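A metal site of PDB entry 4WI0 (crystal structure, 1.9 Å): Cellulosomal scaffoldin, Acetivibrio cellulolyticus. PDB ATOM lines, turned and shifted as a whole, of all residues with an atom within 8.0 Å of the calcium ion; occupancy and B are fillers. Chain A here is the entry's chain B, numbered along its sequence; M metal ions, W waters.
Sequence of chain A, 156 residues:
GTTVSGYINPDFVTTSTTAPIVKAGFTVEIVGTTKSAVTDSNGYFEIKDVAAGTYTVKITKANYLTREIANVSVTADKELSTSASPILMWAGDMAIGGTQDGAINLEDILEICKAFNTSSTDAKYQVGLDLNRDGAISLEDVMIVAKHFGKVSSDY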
ATOM      1  N   LEU A  65       3.350   4.272  10.335  1.00  0.00           N
ATOM      2  CA  LEU A  65       1.892   4.301  10.236  1.00  0.00           C
ATOM      3  C   LEU A  65       1.475   4.939   8.902  1.00  0.00           C
ATOM      4  O   LEU A  65       1.820   6.085   8.600  1.00  0.00           O
ATOM      5  CB  LEU A  65       1.313   5.087  11.410  1.00  0.00           C
ATOM      6  CG  LEU A  65      -0.200   5.080  11.563  1.00  0.00           C
ATOM      7  CD1 LEU A  65      -0.681   3.704  11.995  1.00  0.00           C
ATOM      8  CD2 LEU A  65      -0.596   6.142  12.571  1.00  0.00           C
ATOM      9  N   GLY A  92       6.815   3.514  14.093  1.00  0.00           N
ATOM     10  CA  GLY A  92       6.412   2.664  15.217  1.00  0.00           C
ATOM     11  C   GLY A  92       5.128   1.873  15.068  1.00  0.00           C
ATOM     12  O   GLY A  92       4.660   1.344  16.069  1.00  0.00           O
ATOM     13  N   ASP A  93       4.536   1.811  13.872  1.00  0.00           N
ATOM     14  CA  ASP A  93       3.599   0.727  13.556  1.00  0.00           C
ATOM     15  C   ASP A  93       4.415  -0.398  12.927  1.00  0.00           C
ATOM     16  O   ASP A  93       4.661  -0.415  11.718  1.00  0.00           O
ATOM     17  CB  ASP A  93       2.465   1.170  12.623  1.00  0.00           C
ATOM     18  CG  ASP A  93       1.472   0.042  12.366  1.00  0.00           C
ATOM     19  OD1 ASP A  93       1.442  -0.892  13.182  1.00  0.00           O
ATOM     20  OD2 ASP A  93       0.733   0.077  11.350  1.00  0.00           O
ATOM     21  N   MET A  94       4.816  -1.348  13.775  1.00  0.00           N
ATOM     22  CA  MET A  94       5.835  -2.333  13.445  1.00  0.00           C
ATOM     23  C   MET A  94       5.260  -3.562  12.740  1.00  0.00           C
ATOM     24  O   MET A  94       4.137  -3.977  13.022  1.00  0.00           O
ATOM     25  CB  MET A  94       6.530  -2.788  14.729  1.00  0.00           C
ATOM     26  CG  MET A  94       7.065  -1.672  15.606  1.00  0.00           C
ATOM     27  SD  MET A  94       8.241  -0.604  14.767  1.00  0.00           S
ATOM     28  CE  MET A  94       9.612  -1.735  14.599  1.00  0.00           C
ATOM     29  N   ALA A  95       6.054  -4.142  11.840  1.00  0.00           N
ATOM     30  CA  ALA A  95       5.723  -5.434  11.236  1.00  0.00           C
ATOM     31  C   ALA A  95       5.862  -6.554  12.263  1.00  0.00           C
ATOM     32  O   ALA A  95       6.967  -6.925  12.661  1.00  0.00           O
ATOM     33  CB  ALA A  95       6.595  -5.699  10.019  1.00  0.00           C
ATOM     34  N   ILE A  96       4.709  -7.091  12.692  1.00  0.00           N
ATOM     35  CA  ILE A  96       4.645  -8.160  13.682  1.00  0.00           C
ATOM     36  C   ILE A  96       3.842  -9.288  13.056  1.00  0.00           C
ATOM     37  O   ILE A  96       2.697  -9.084  12.644  1.00  0.00           O
ATOM     38  CB  ILE A  96       3.942  -7.690  14.989  1.00  0.00           C
ATOM     39  CG1 ILE A  96       4.648  -6.448  15.561  1.00  0.00           C
ATOM     40  CG2 ILE A  96       3.947  -8.812  16.026  1.00  0.00           C
ATOM     41  CD1 ILE A  96       3.841  -5.735  16.631  1.00  0.00           C
ATOM     42  N   THR A  99       3.219  -8.406   9.298  1.00  0.00           N
ATOM     43  CA  THR A  99       2.127  -7.481   8.976  1.00  0.00           C
ATOM     44  C   THR A  99       1.985  -6.355  10.006  1.00  0.00           C
ATOM     45  O   THR A  99       2.105  -6.583  11.208  1.00  0.00           O
ATOM     46  CB  THR A  99       0.783  -8.224   8.894  1.00  0.00           C
ATOM     47  OG1 THR A  99       0.910  -9.329   8.010  1.00  0.00           O
ATOM     48  CG2 THR A  99      -0.323  -7.296   8.395  1.00  0.00           C
ATOM     49  N   GLN A 100       1.716  -5.146   9.503  1.00  0.00           N
ATOM     50  CA  GLN A 100       1.388  -4.000  10.347  1.00  0.00           C
ATOM     51  C   GLN A 100      -0.118  -3.943  10.540  1.00  0.00           C
ATOM     52  O   GLN A 100      -0.869  -4.364   9.670  1.00  0.00           O
ATOM     53  CB  GLN A 100       1.879  -2.721   9.703  1.00  0.00           C
ATOM     54  CG  GLN A 100       3.390  -2.669   9.544  1.00  0.00           C
ATOM     55  CD  GLN A 100       3.874  -1.427   8.815  1.00  0.00           C
ATOM     56  OE1 GLN A 100       4.841  -1.487   8.071  1.00  0.00           O
ATOM     57  NE2 GLN A 100       3.215  -0.305   9.036  1.00  0.00           N
ATOM     58  N   ASP A 101      -0.572  -3.405  11.670  1.00  0.00           N
ATOM     59  CA  ASP A 101      -2.006  -3.392  11.975  1.00  0.00           C
ATOM     60  C   ASP A 101      -2.633  -1.991  11.950  1.00  0.00           C
ATOM     61  O   ASP A 101      -3.811  -1.844  12.267  1.00  0.00           O
ATOM     62  CB  ASP A 101      -2.278  -4.090  13.316  1.00  0.00           C
ATOM     63  CG  ASP A 101      -1.690  -3.355  14.511  1.00  0.00           C
ATOM     64  OD1 ASP A 101      -1.002  -2.344  14.303  1.00  0.00           O
ATOM     65  OD2 ASP A 101      -1.923  -3.792  15.662  1.00  0.00           O
ATOM     66  N   GLY A 102      -1.866  -0.968  11.575  1.00  0.00           N
ATOM     67  CA  GLY A 102      -2.407   0.391  11.448  1.00  0.00           C
ATOM     68  C   GLY A 102      -2.763   1.045  12.778  1.00  0.00           C
ATOM     69  O   GLY A 102      -3.641   1.903  12.857  1.00  0.00           O
ATOM     70  N   ALA A 103      -2.089   0.609  13.839  1.00  0.00           N
ATOM     71  CA  ALA A 103      -2.189   1.228  15.138  1.00  0.00           C
ATOM     72  C   ALA A 103      -0.800   1.258  15.764  1.00  0.00           C
ATOM     73  O   ALA A 103       0.008   0.350  15.533  1.00  0.00           O
ATOM     74  CB  ALA A 103      -3.135   0.438  16.028  1.00  0.00           C
ATOM     75  N   ILE A 104      -0.527   2.308  16.525  1.00  0.00           N
ATOM     76  CA  ILE A 104       0.686   2.385  17.331  1.00  0.00           C
ATOM     77  C   ILE A 104       0.287   2.150  18.783  1.00  0.00           C
ATOM     78  O   ILE A 104      -0.380   2.985  19.382  1.00  0.00           O
ATOM     79  CB  ILE A 104       1.367   3.754  17.183  1.00  0.00           C
ATOM     80  CG1 ILE A 104       1.880   3.914  15.743  1.00  0.00           C
ATOM     81  CG2 ILE A 104       2.512   3.903  18.171  1.00  0.00           C
ATOM     82  CD1 ILE A 104       2.457   5.273  15.428  1.00  0.00           C
ATOM     83  N   ASN A 105       0.678   1.006  19.339  1.00  0.00           N
ATOM     84  CA  ASN A 105       0.264   0.647  20.702  1.00  0.00           C
ATOM     85  C   ASN A 105       1.362  -0.142  21.447  1.00  0.00           C
ATOM     86  O   ASN A 105       2.534  -0.096  21.042  1.00  0.00           O
ATOM     87  CB  ASN A 105      -1.087  -0.092  20.665  1.00  0.00           C
ATOM     88  CG  ASN A 105      -1.079  -1.304  19.756  1.00  0.00           C
ATOM     89  OD1 ASN A 105      -0.073  -1.999  19.613  1.00  0.00           O
ATOM     90  ND2 ASN A 105      -2.240  -1.594  19.161  1.00  0.00           N
ATOM     91  N   LEU A 106       0.995  -0.834  22.519  1.00  0.00           N
ATOM     92  CA  LEU A 106       1.966  -1.546  23.361  1.00  0.00           C
ATOM     93  C   LEU A 106       2.722  -2.641  22.604  1.00  0.00           C
ATOM     94  O   LEU A 106       3.906  -2.849  22.838  1.00  0.00           O
ATOM     95  CB  LEU A 106       1.283  -2.140  24.587  1.00  0.00           C
ATOM     96  CG  LEU A 106       2.152  -2.796  25.665  1.00  0.00           C
ATOM     97  CD1 LEU A 106       3.069  -1.772  26.325  1.00  0.00           C
ATOM     98  CD2 LEU A 106       1.294  -3.485  26.699  1.00  0.00           C
ATOM     99  N   GLU A 107       2.028  -3.327  21.695  1.00  0.00           N
ATOM    100  CA  GLU A 107       2.644  -4.437  20.944  1.00  0.00           C
ATOM    101  C   GLU A 107       3.823  -3.958  20.112  1.00  0.00           C
ATOM    102  O   GLU A 107       4.820  -4.656  19.969  1.00  0.00           O
ATOM    103  CB  GLU A 107       1.624  -5.143  20.049  1.00  0.00           C
ATOM    104  CG  GLU A 107       0.789  -6.203  20.762  1.00  0.00           C
ATOM    105  CD  GLU A 107       0.050  -5.670  21.957  1.00  0.00           C
ATOM    106  OE1 GLU A 107      -0.826  -4.777  21.781  1.00  0.00           O
ATOM    107  OE2 GLU A 107       0.330  -6.127  23.083  1.00  0.00           O
ATOM    108  N   ASP A 108       3.685  -2.747  19.568  1.00  0.00           N
ATOM    109  CA  ASP A 108       4.755  -2.111  18.802  1.00  0.00           C
ATOM    110  C   ASP A 108       5.948  -1.821  19.699  1.00  0.00           C
ATOM    111  O   ASP A 108       7.097  -2.070  19.312  1.00  0.00           O
ATOM    112  CB  ASP A 108       4.249  -0.834  18.157  1.00  0.00           C
ATOM    113  CG  ASP A 108       3.155  -1.097  17.157  1.00  0.00           C
ATOM    114  OD1 ASP A 108       3.436  -1.735  16.130  1.00  0.00           O
ATOM    115  OD2 ASP A 108       2.013  -0.678  17.406  1.00  0.00           O
ATOM    116  N   ILE A 109       5.671  -1.304  20.889  1.00  0.00           N
ATOM    117  CA  ILE A 109       6.723  -1.076  21.895  1.00  0.00           C
ATOM    118  C   ILE A 109       7.376  -2.393  22.292  1.00  0.00           C
ATOM    119  O   ILE A 109       8.599  -2.482  22.367  1.00  0.00           O
ATOM    120  CB  ILE A 109       6.182  -0.369  23.165  1.00  0.00           C
ATOM    121  CG1 ILE A 109       5.769   1.069  22.809  1.00  0.00           C
ATOM    122  CG2 ILE A 109       7.234  -0.383  24.275  1.00  0.00           C
ATOM    123  CD1 ILE A 109       5.448   1.973  23.979  1.00  0.00           C
ATOM    124  N   VAL A 145       8.048   5.959  19.480  1.00  0.00           N
ATOM    125  CA  VAL A 145       6.756   5.290  19.381  1.00  0.00           C
ATOM    126  C   VAL A 145       5.778   5.954  20.347  1.00  0.00           C
ATOM    127  O   VAL A 145       4.643   6.251  19.984  1.00  0.00           O
ATOM    128  CB  VAL A 145       6.874   3.771  19.673  1.00  0.00           C
ATOM    129  CG1 VAL A 145       5.523   3.085  19.547  1.00  0.00           C
ATOM    130  CG2 VAL A 145       7.872   3.115  18.727  1.00  0.00           C
ATOM    131  N   LYS A 151      -2.440   5.800  18.732  1.00  0.00           N
ATOM    132  CA  LYS A 151      -2.988   6.418  17.518  1.00  0.00           C
ATOM    133  C   LYS A 151      -3.156   5.439  16.349  1.00  0.00           C
ATOM    134  O   LYS A 151      -2.503   4.386  16.299  1.00  0.00           O
ATOM    135  CB  LYS A 151      -2.100   7.586  17.063  1.00  0.00           C
ATOM    136  CG  LYS A 151      -1.992   8.734  18.049  1.00  0.00           C
ATOM    137  CD  LYS A 151      -3.317   9.468  18.234  1.00  0.00           C
ATOM    138  CE  LYS A 151      -3.327  10.320  19.486  1.00  0.00           C
ATOM    139  NZ  LYS A 151      -3.220   9.495  20.738  1.00  0.00           N
HETATM  140 CA    CA M   1       1.020  -1.656  15.352  1.00  0.00          CA
HETATM  141  O   HOH W   1       1.663  -3.715  14.195  1.00  0.00           O
HETATM  142  O   HOH W   2       0.329  -3.163  17.068  1.00  0.00           O
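Four residues have an atom within 4 Å of the calcium ion: Asp 93, Asp 101, Ala 103 and Asp 108.
The backbone carbonyl oxygen (O) of Asp 93 is in hydrogen-bond range of the side-chain amide nitrogen (NE2) of Gln 100, at 3.0 Å. The backbone NH (N) of Gly 102 lies within hydrogen-bond range of the side-chain carboxylate (OD2) of Asp 93, 2.8 Å away. The backbone NH of Asn 105 sits close to the side-chain carboxylate of Asp 108, at 2.9 Å. OD1 of Asp 108 lies close to N of Met 94 (2.8 Å).
Water W2 lies within hydrogen-bond range of the side-chain carboxylate (OD2) of Asp 101 (2.7 Å) and the side-chain amide oxygen (OD1) of Asn 105 (2.8 Å). Water W1 lies within hydrogen-bond range of O of Met 94 and N of Asp 101.
The calcium ion is bound by the backbone carbonyl oxygen (O) of Ala 103, the side-chain carboxylate (OD1) of Asp 93, the side-chain carboxylate (OD1) of Asp 101, water W2, water W1, the side-chain carboxylate (OD2) of Asp 108 and the side-chain carboxylate (OD1) of Asp 108. The calcium ion has seven donor atoms within binding distance.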
